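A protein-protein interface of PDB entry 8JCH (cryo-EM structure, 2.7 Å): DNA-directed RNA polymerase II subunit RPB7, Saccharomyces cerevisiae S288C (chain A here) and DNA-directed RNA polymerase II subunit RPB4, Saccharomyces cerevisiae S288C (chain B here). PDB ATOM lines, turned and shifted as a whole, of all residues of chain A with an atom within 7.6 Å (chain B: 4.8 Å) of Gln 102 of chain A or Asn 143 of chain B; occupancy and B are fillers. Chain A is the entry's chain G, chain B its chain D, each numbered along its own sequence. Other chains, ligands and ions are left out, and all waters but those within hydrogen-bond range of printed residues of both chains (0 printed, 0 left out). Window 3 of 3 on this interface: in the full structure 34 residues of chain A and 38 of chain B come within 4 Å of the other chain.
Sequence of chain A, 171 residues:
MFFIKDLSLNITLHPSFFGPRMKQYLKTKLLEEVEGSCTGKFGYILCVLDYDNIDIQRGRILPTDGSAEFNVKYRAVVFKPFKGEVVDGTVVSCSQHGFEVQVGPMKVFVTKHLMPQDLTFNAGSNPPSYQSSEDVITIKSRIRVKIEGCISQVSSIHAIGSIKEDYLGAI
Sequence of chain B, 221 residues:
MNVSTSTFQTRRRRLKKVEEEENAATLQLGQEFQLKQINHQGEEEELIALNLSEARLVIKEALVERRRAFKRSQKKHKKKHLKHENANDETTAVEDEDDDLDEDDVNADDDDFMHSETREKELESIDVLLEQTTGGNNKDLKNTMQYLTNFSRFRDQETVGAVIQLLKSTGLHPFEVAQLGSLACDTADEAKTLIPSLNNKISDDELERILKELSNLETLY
OE1 of Gln 102 of chain A sits close to O of Gly 104 of chain A, at 2.9 Å.
O of Lys 139 of chain B sits close to OD1 of Asn 143 of chain B.
OE1 of Gln 102 of chain A lies close to O of Met 106 of chain A (2.8 Å).
The backbone carbonyl oxygen (O) of Leu 141 of chain B sits at hydrogen-bond distance from the side-chain hydroxyl (OG1) of Thr 144 of chain B (2.8 Å).
O of Thr 90 of chain A sits at hydrogen-bond distance from N of Gln 102 of chain A (2.6 Å).
Asp 88 of chain A touches Tyr 147 of chain B.
Gln 102 of chain A touches Asn 143 of chain B (NE2 to ND2, 3.97 Å).
Gly 104 of chain A touches Tyr 147 of chain B (N to CD2, 3.8 Å).
Asp 140 of chain B touches Pro 105 of chain A.
Thr 144 of chain B touches Pro 105 of chain A.
Of chain B, only Asn 143 (3.97 Å) comes within 4 Å of Gln 102 of chain A.
Of chain A, only Gln 102 comes within 4 Å of Asn 143 of chain B.
Printed residues of chain B within 4 Å of Gly 104 of chain A: Tyr 147.
Of the printed residues of chain A, Thr 144 of chain B touches Pro 105 (3.6 Å).
Of the printed residues of chain A, Tyr 147 of chain B touches Asp 88 (3.2 Å) and Gly 104 (3.8 Å).
Of the printed residues of chain B, Asp 88 of chain A touches Tyr 147 (3.2 Å).
Thr 90 of chain A touches none of the printed residues of chain B.
The nearest residue of chain B that does not touch Gln 102 of chain A is Tyr 147 of chain B (4.4 Å).
Of the 19 printed residues of chain A, 4 touch a printed residue of chain B.
Printed residues of chain A that touch a printed residue of chain B: Asp 88, Gln 102, Gly 104 and Pro 105.
Hydrophobic or aromatic side chains of chain A within 4 Å of the printed part of chain B: Pro 105.
Among the printed residues, no Asp or Glu carboxylate lies within 4 Å of a Lys or Arg side-chain nitrogen of the other chain.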
ATOM      1  N   ASP A  88     -22.565  -9.417  17.592  1.00  0.00           N
ATOM      2  CA  ASP A  88     -23.553  -9.381  18.661  1.00  0.00           C
ATOM      3  C   ASP A  88     -24.031  -7.950  18.857  1.00  0.00           C
ATOM      4  O   ASP A  88     -23.216  -7.024  18.922  1.00  0.00           O
ATOM      5  CB  ASP A  88     -22.973  -9.932  19.967  1.00  0.00           C
ATOM      6  CG  ASP A  88     -21.480  -9.690  20.091  1.00  0.00           C
ATOM      7  OD1 ASP A  88     -20.791  -9.667  19.051  1.00  0.00           O
ATOM      8  OD2 ASP A  88     -20.997  -9.524  21.231  1.00  0.00           O
ATOM      9  N   GLY A  89     -25.346  -7.775  18.952  1.00  0.00           N
ATOM     10  CA  GLY A  89     -25.921  -6.456  19.131  1.00  0.00           C
ATOM     11  C   GLY A  89     -27.162  -6.451  20.000  1.00  0.00           C
ATOM     12  O   GLY A  89     -27.385  -7.380  20.784  1.00  0.00           O
ATOM     13  N   THR A  90     -27.978  -5.408  19.870  1.00  0.00           N
ATOM     14  CA  THR A  90     -29.199  -5.264  20.648  1.00  0.00           C
ATOM     15  C   THR A  90     -30.358  -4.918  19.723  1.00  0.00           C
ATOM     16  O   THR A  90     -30.176  -4.276  18.686  1.00  0.00           O
ATOM     17  CB  THR A  90     -29.058  -4.181  21.727  1.00  0.00           C
ATOM     18  OG1 THR A  90     -28.316  -3.074  21.202  1.00  0.00           O
ATOM     19  CG2 THR A  90     -28.336  -4.736  22.946  1.00  0.00           C
ATOM     20  N   VAL A  91     -31.551  -5.353  20.111  1.00  0.00           N
ATOM     21  CA  VAL A  91     -32.751  -5.104  19.320  1.00  0.00           C
ATOM     22  C   VAL A  91     -33.244  -3.690  19.591  1.00  0.00           C
ATOM     23  O   VAL A  91     -33.354  -3.268  20.749  1.00  0.00           O
ATOM     24  CB  VAL A  91     -33.838  -6.143  19.637  1.00  0.00           C
ATOM     25  CG1 VAL A  91     -34.962  -6.062  18.616  1.00  0.00           C
ATOM     26  CG2 VAL A  91     -33.240  -7.540  19.672  1.00  0.00           C
ATOM     27  N   VAL A  92     -33.542  -2.954  18.525  1.00  0.00           N
ATOM     28  CA  VAL A  92     -34.031  -1.583  18.616  1.00  0.00           C
ATOM     29  C   VAL A  92     -35.465  -1.470  18.109  1.00  0.00           C
ATOM     30  O   VAL A  92     -36.336  -0.935  18.797  1.00  0.00           O
ATOM     31  CB  VAL A  92     -33.097  -0.613  17.859  1.00  0.00           C
ATOM     32  CG1 VAL A  92     -33.799   0.711  17.597  1.00  0.00           C
ATOM     33  CG2 VAL A  92     -31.815  -0.394  18.644  1.00  0.00           C
ATOM     34  N   SER A  93     -35.728  -1.975  16.907  1.00  0.00           N
ATOM     35  CA  SER A  93     -37.054  -1.931  16.311  1.00  0.00           C
ATOM     36  C   SER A  93     -37.465  -3.331  15.882  1.00  0.00           C
ATOM     37  O   SER A  93     -36.622  -4.165  15.538  1.00  0.00           O
ATOM     38  CB  SER A  93     -37.098  -0.979  15.107  1.00  0.00           C
ATOM     39  OG  SER A  93     -36.049  -0.029  15.170  1.00  0.00           O
ATOM     40  N   PHE A  99     -37.067  -8.180  13.118  1.00  0.00           N
ATOM     41  CA  PHE A  99     -36.480  -7.445  14.229  1.00  0.00           C
ATOM     42  C   PHE A  99     -35.086  -6.969  13.843  1.00  0.00           C
ATOM     43  O   PHE A  99     -34.278  -7.745  13.322  1.00  0.00           O
ATOM     44  CB  PHE A  99     -36.440  -8.306  15.499  1.00  0.00           C
ATOM     45  CG  PHE A  99     -35.261  -9.233  15.579  1.00  0.00           C
ATOM     46  CD1 PHE A  99     -35.236 -10.407  14.847  1.00  0.00           C
ATOM     47  CD2 PHE A  99     -34.180  -8.935  16.394  1.00  0.00           C
ATOM     48  CE1 PHE A  99     -34.156 -11.266  14.922  1.00  0.00           C
ATOM     49  CE2 PHE A  99     -33.097  -9.789  16.472  1.00  0.00           C
ATOM     50  CZ  PHE A  99     -33.085 -10.955  15.735  1.00  0.00           C
ATOM     51  N   GLU A 100     -34.822  -5.685  14.072  1.00  0.00           N
ATOM     52  CA  GLU A 100     -33.541  -5.084  13.741  1.00  0.00           C
ATOM     53  C   GLU A 100     -32.546  -5.265  14.885  1.00  0.00           C
ATOM     54  O   GLU A 100     -32.906  -5.603  16.015  1.00  0.00           O
ATOM     55  CB  GLU A 100     -33.705  -3.596  13.412  1.00  0.00           C
ATOM     56  CG  GLU A 100     -34.276  -3.256  12.022  1.00  0.00           C
ATOM     57  CD  GLU A 100     -35.717  -3.704  11.779  1.00  0.00           C
ATOM     58  OE1 GLU A 100     -36.383  -3.077  10.929  1.00  0.00           O
ATOM     59  OE2 GLU A 100     -36.202  -4.654  12.428  1.00  0.00           O
ATOM     60  N   VAL A 101     -31.271  -5.030  14.574  1.00  0.00           N
ATOM     61  CA  VAL A 101     -30.183  -5.177  15.528  1.00  0.00           C
ATOM     62  C   VAL A 101     -29.389  -3.877  15.533  1.00  0.00           C
ATOM     63  O   VAL A 101     -29.421  -3.098  14.577  1.00  0.00           O
ATOM     64  CB  VAL A 101     -29.274  -6.383  15.192  1.00  0.00           C
ATOM     65  CG1 VAL A 101     -28.333  -6.704  16.345  1.00  0.00           C
ATOM     66  CG2 VAL A 101     -30.110  -7.604  14.830  1.00  0.00           C
ATOM     67  N   GLN A 102     -28.671  -3.643  16.633  1.00  0.00           N
ATOM     68  CA  GLN A 102     -27.922  -2.405  16.809  1.00  0.00           C
ATOM     69  C   GLN A 102     -26.429  -2.697  16.914  1.00  0.00           C
ATOM     70  O   GLN A 102     -25.743  -2.177  17.799  1.00  0.00           O
ATOM     71  CB  GLN A 102     -28.425  -1.655  18.050  1.00  0.00           C
ATOM     72  CG  GLN A 102     -27.977  -0.184  18.250  1.00  0.00           C
ATOM     73  CD  GLN A 102     -27.930   0.670  16.983  1.00  0.00           C
ATOM     74  OE1 GLN A 102     -27.269   0.337  15.999  1.00  0.00           O
ATOM     75  NE2 GLN A 102     -28.642   1.790  17.013  1.00  0.00           N
ATOM     76  N   VAL A 103     -25.921  -3.545  16.023  1.00  0.00           N
ATOM     77  CA  VAL A 103     -24.488  -3.824  15.973  1.00  0.00           C
ATOM     78  C   VAL A 103     -23.780  -2.562  15.494  1.00  0.00           C
ATOM     79  O   VAL A 103     -23.901  -2.176  14.327  1.00  0.00           O
ATOM     80  CB  VAL A 103     -24.175  -5.017  15.062  1.00  0.00           C
ATOM     81  CG1 VAL A 103     -22.673  -5.161  14.880  1.00  0.00           C
ATOM     82  CG2 VAL A 103     -24.770  -6.292  15.635  1.00  0.00           C
ATOM     83  N   GLY A 104     -23.038  -1.917  16.390  1.00  0.00           N
ATOM     84  CA  GLY A 104     -22.367  -0.679  16.073  1.00  0.00           C
ATOM     85  C   GLY A 104     -23.347   0.421  15.726  1.00  0.00           C
ATOM     86  O   GLY A 104     -24.430   0.529  16.309  1.00  0.00           O
ATOM     87  N   PRO A 105     -22.983   1.266  14.763  1.00  0.00           N
ATOM     88  CA  PRO A 105     -23.879   2.341  14.315  1.00  0.00           C
ATOM     89  C   PRO A 105     -24.817   1.963  13.176  1.00  0.00           C
ATOM     90  O   PRO A 105     -25.418   2.862  12.581  1.00  0.00           O
ATOM     91  CB  PRO A 105     -22.884   3.411  13.850  1.00  0.00           C
ATOM     92  CG  PRO A 105     -21.717   2.624  13.328  1.00  0.00           C
ATOM     93  CD  PRO A 105     -21.690   1.297  14.058  1.00  0.00           C
ATOM     94  N   MET A 106     -24.956   0.679  12.860  1.00  0.00           N
ATOM     95  CA  MET A 106     -25.708   0.235  11.699  1.00  0.00           C
ATOM     96  C   MET A 106     -27.146  -0.109  12.083  1.00  0.00           C
ATOM     97  O   MET A 106     -27.565   0.016  13.235  1.00  0.00           O
ATOM     98  CB  MET A 106     -25.014  -0.964  11.052  1.00  0.00           C
ATOM     99  CG  MET A 106     -23.753  -0.604  10.292  1.00  0.00           C
ATOM    100  SD  MET A 106     -22.827  -2.062   9.791  1.00  0.00           S
ATOM    101  CE  MET A 106     -22.447  -2.786  11.384  1.00  0.00           C
ATOM    102  N   LYS A 107     -27.910  -0.551  11.086  1.00  0.00           N
ATOM    103  CA  LYS A 107     -29.315  -0.918  11.229  1.00  0.00           C
ATOM    104  C   LYS A 107     -29.580  -2.253  10.546  1.00  0.00           C
ATOM    105  O   LYS A 107     -30.499  -2.397   9.735  1.00  0.00           O
ATOM    106  CB  LYS A 107     -30.225   0.171  10.667  1.00  0.00           C
ATOM    107  CG  LYS A 107     -30.145   1.496  11.407  1.00  0.00           C
ATOM    108  CD  LYS A 107     -31.527   2.080  11.648  1.00  0.00           C
ATOM    109  CE  LYS A 107     -31.488   3.172  12.706  1.00  0.00           C
ATOM    110  NZ  LYS A 107     -32.855   3.561  13.153  1.00  0.00           N
ATOM    111  N   VAL A 108     -28.744  -3.249  10.858  1.00  0.00           N
ATOM    112  CA  VAL A 108     -28.851  -4.559  10.225  1.00  0.00           C
ATOM    113  C   VAL A 108     -30.238  -5.138  10.460  1.00  0.00           C
ATOM    114  O   VAL A 108     -30.745  -5.152  11.590  1.00  0.00           O
ATOM    115  CB  VAL A 108     -27.750  -5.492  10.751  1.00  0.00           C
ATOM    116  CG1 VAL A 108     -27.413  -5.152  12.195  1.00  0.00           C
ATOM    117  CG2 VAL A 108     -28.166  -6.950  10.623  1.00  0.00           C
ATOM    118  N   SER A 141     -32.325  -6.413  24.009  1.00  0.00           N
ATOM    119  CA  SER A 141     -31.859  -7.667  24.577  1.00  0.00           C
ATOM    120  C   SER A 141     -30.678  -8.184  23.772  1.00  0.00           C
ATOM    121  O   SER A 141     -30.523  -7.862  22.590  1.00  0.00           O
ATOM    122  CB  SER A 141     -32.974  -8.721  24.608  1.00  0.00           C
ATOM    123  OG  SER A 141     -32.444 -10.018  24.817  1.00  0.00           O
ATOM    124  N   ILE A 143     -28.399 -10.343  21.502  1.00  0.00           N
ATOM    125  CA  ILE A 143     -28.684 -11.171  20.335  1.00  0.00           C
ATOM    126  C   ILE A 143     -27.445 -11.190  19.451  1.00  0.00           C
ATOM    127  O   ILE A 143     -26.831 -10.150  19.194  1.00  0.00           O
ATOM    128  CB  ILE A 143     -29.929 -10.658  19.573  1.00  0.00           C
ATOM    129  CG1 ILE A 143     -30.083 -11.385  18.236  1.00  0.00           C
ATOM    130  CG2 ILE A 143     -29.856  -9.151  19.371  1.00  0.00           C
ATOM    131  CD1 ILE A 143     -30.408 -12.857  18.374  1.00  0.00           C
ATOM    132  N   VAL A 145     -26.077 -12.070  15.701  1.00  0.00           N
ATOM    133  CA  VAL A 145     -26.637 -12.104  14.356  1.00  0.00           C
ATOM    134  C   VAL A 145     -25.501 -12.127  13.341  1.00  0.00           C
ATOM    135  O   VAL A 145     -24.513 -11.398  13.482  1.00  0.00           O
ATOM    136  CB  VAL A 145     -27.573 -10.900  14.113  1.00  0.00           C
ATOM    137  CG1 VAL A 145     -26.902  -9.601  14.536  1.00  0.00           C
ATOM    138  CG2 VAL A 145     -28.006 -10.835  12.661  1.00  0.00           C
ATOM    139  N   LYS B 139     -23.288  12.541  16.113  1.00  0.00           N
ATOM    140  CA  LYS B 139     -24.384  11.637  16.451  1.00  0.00           C
ATOM    141  C   LYS B 139     -23.961  10.179  16.327  1.00  0.00           C
ATOM    142  O   LYS B 139     -24.348   9.343  17.150  1.00  0.00           O
ATOM    143  CB  LYS B 139     -25.592  11.923  15.560  1.00  0.00           C
ATOM    144  CG  LYS B 139     -26.861  11.201  15.982  1.00  0.00           C
ATOM    145  CD  LYS B 139     -27.180  11.452  17.448  1.00  0.00           C
ATOM    146  CE  LYS B 139     -28.389  10.645  17.895  1.00  0.00           C
ATOM    147  NZ  LYS B 139     -28.718  10.888  19.327  1.00  0.00           N
ATOM    148  N   ASP B 140     -23.165   9.856  15.304  1.00  0.00           N
ATOM    149  CA  ASP B 140     -22.777   8.468  15.071  1.00  0.00           C
ATOM    150  C   ASP B 140     -21.841   7.947  16.154  1.00  0.00           C
ATOM    151  O   ASP B 140     -21.828   6.742  16.430  1.00  0.00           O
ATOM    152  CB  ASP B 140     -22.124   8.336  13.695  1.00  0.00           C
ATOM    153  CG  ASP B 140     -21.911   6.893  13.286  1.00  0.00           C
ATOM    154  OD1 ASP B 140     -20.904   6.292  13.714  1.00  0.00           O
ATOM    155  OD2 ASP B 140     -22.752   6.359  12.532  1.00  0.00           O
ATOM    156  N   LEU B 141     -21.054   8.830  16.774  1.00  0.00           N
ATOM    157  CA  LEU B 141     -20.069   8.384  17.754  1.00  0.00           C
ATOM    158  C   LEU B 141     -20.723   7.845  19.021  1.00  0.00           C
ATOM    159  O   LEU B 141     -20.162   6.956  19.672  1.00  0.00           O
ATOM    160  CB  LEU B 141     -19.117   9.530  18.097  1.00  0.00           C
ATOM    161  CG  LEU B 141     -17.715   9.158  18.587  1.00  0.00           C
ATOM    162  CD1 LEU B 141     -17.659   9.138  20.108  1.00  0.00           C
ATOM    163  CD2 LEU B 141     -17.267   7.821  18.012  1.00  0.00           C
ATOM    164  N   LYS B 142     -21.895   8.368  19.389  1.00  0.00           N
ATOM    165  CA  LYS B 142     -22.541   7.944  20.629  1.00  0.00           C
ATOM    166  C   LYS B 142     -22.917   6.467  20.580  1.00  0.00           C
ATOM    167  O   LYS B 142     -22.671   5.720  21.536  1.00  0.00           O
ATOM    168  CB  LYS B 142     -23.778   8.803  20.894  1.00  0.00           C
ATOM    169  CG  LYS B 142     -23.541  10.297  20.757  1.00  0.00           C
ATOM    170  CD  LYS B 142     -24.840  11.076  20.878  1.00  0.00           C
ATOM    171  CE  LYS B 142     -24.587  12.575  20.888  1.00  0.00           C
ATOM    172  NZ  LYS B 142     -25.856  13.353  20.929  1.00  0.00           N
ATOM    173  N   ASN B 143     -23.513   6.027  19.469  1.00  0.00           N
ATOM    174  CA  ASN B 143     -23.952   4.638  19.364  1.00  0.00           C
ATOM    175  C   ASN B 143     -22.772   3.677  19.392  1.00  0.00           C
ATOM    176  O   ASN B 143     -22.838   2.625  20.040  1.00  0.00           O
ATOM    177  CB  ASN B 143     -24.775   4.442  18.093  1.00  0.00           C
ATOM    178  CG  ASN B 143     -25.677   5.622  17.794  1.00  0.00           C
ATOM    179  OD1 ASN B 143     -25.236   6.771  17.798  1.00  0.00           O
ATOM    180  ND2 ASN B 143     -26.949   5.345  17.535  1.00  0.00           N
ATOM    181  N   THR B 144     -21.685   4.015  18.694  1.00  0.00           N
ATOM    182  CA  THR B 144     -20.518   3.138  18.667  1.00  0.00           C
ATOM    183  C   THR B 144     -19.915   2.986  20.058  1.00  0.00           C
ATOM    184  O   THR B 144     -19.586   1.873  20.488  1.00  0.00           O
ATOM    185  CB  THR B 144     -19.476   3.678  17.690  1.00  0.00           C
ATOM    186  OG1 THR B 144     -18.942   4.909  18.192  1.00  0.00           O
ATOM    187  CG2 THR B 144     -20.104   3.926  16.329  1.00  0.00           C
ATOM    188  N   MET B 145     -19.766   4.099  20.780  1.00  0.00           N
ATOM    189  CA  MET B 145     -19.193   4.034  22.121  1.00  0.00           C
ATOM    190  C   MET B 145     -20.114   3.288  23.077  1.00  0.00           C
ATOM    191  O   MET B 145     -19.646   2.520  23.926  1.00  0.00           O
ATOM    192  CB  MET B 145     -18.906   5.446  22.637  1.00  0.00           C
ATOM    193  CG  MET B 145     -17.426   5.878  22.657  1.00  0.00           C
ATOM    194  SD  MET B 145     -16.080   4.698  22.974  1.00  0.00           S
ATOM    195  CE  MET B 145     -16.687   3.694  24.332  1.00  0.00           C
ATOM    196  N   GLN B 146     -21.428   3.499  22.954  1.00  0.00           N
ATOM    197  CA  GLN B 146     -22.372   2.775  23.799  1.00  0.00           C
ATOM    198  C   GLN B 146     -22.305   1.274  23.540  1.00  0.00           C
ATOM    199  O   GLN B 146     -22.319   0.472  24.480  1.00  0.00           O
ATOM    200  CB  GLN B 146     -23.790   3.299  23.568  1.00  0.00           C
ATOM    201  CG  GLN B 146     -24.648   3.345  24.821  1.00  0.00           C
ATOM    202  CD  GLN B 146     -25.706   2.259  24.841  1.00  0.00           C
ATOM    203  OE1 GLN B 146     -25.742   1.395  23.964  1.00  0.00           O
ATOM    204  NE2 GLN B 146     -26.575   2.297  25.843  1.00  0.00           N
ATOM    205  N   TYR B 147     -22.229   0.878  22.266  1.00  0.00           N
ATOM    206  CA  TYR B 147     -22.121  -0.539  21.935  1.00  0.00           C
ATOM    207  C   TYR B 147     -20.809  -1.124  22.442  1.00  0.00           C
ATOM    208  O   TYR B 147     -20.774  -2.262  22.924  1.00  0.00           O
ATOM    209  CB  TYR B 147     -22.252  -0.732  20.424  1.00  0.00           C
ATOM    210  CG  TYR B 147     -21.612  -1.997  19.901  1.00  0.00           C
ATOM    211  CD1 TYR B 147     -22.174  -3.241  20.156  1.00  0.00           C
ATOM    212  CD2 TYR B 147     -20.447  -1.949  19.147  1.00  0.00           C
ATOM    213  CE1 TYR B 147     -21.594  -4.399  19.679  1.00  0.00           C
ATOM    214  CE2 TYR B 147     -19.860  -3.102  18.665  1.00  0.00           C
ATOM    215  CZ  TYR B 147     -20.436  -4.324  18.933  1.00  0.00           C
ATOM    216  OH  TYR B 147     -19.854  -5.475  18.456  1.00  0.00           O
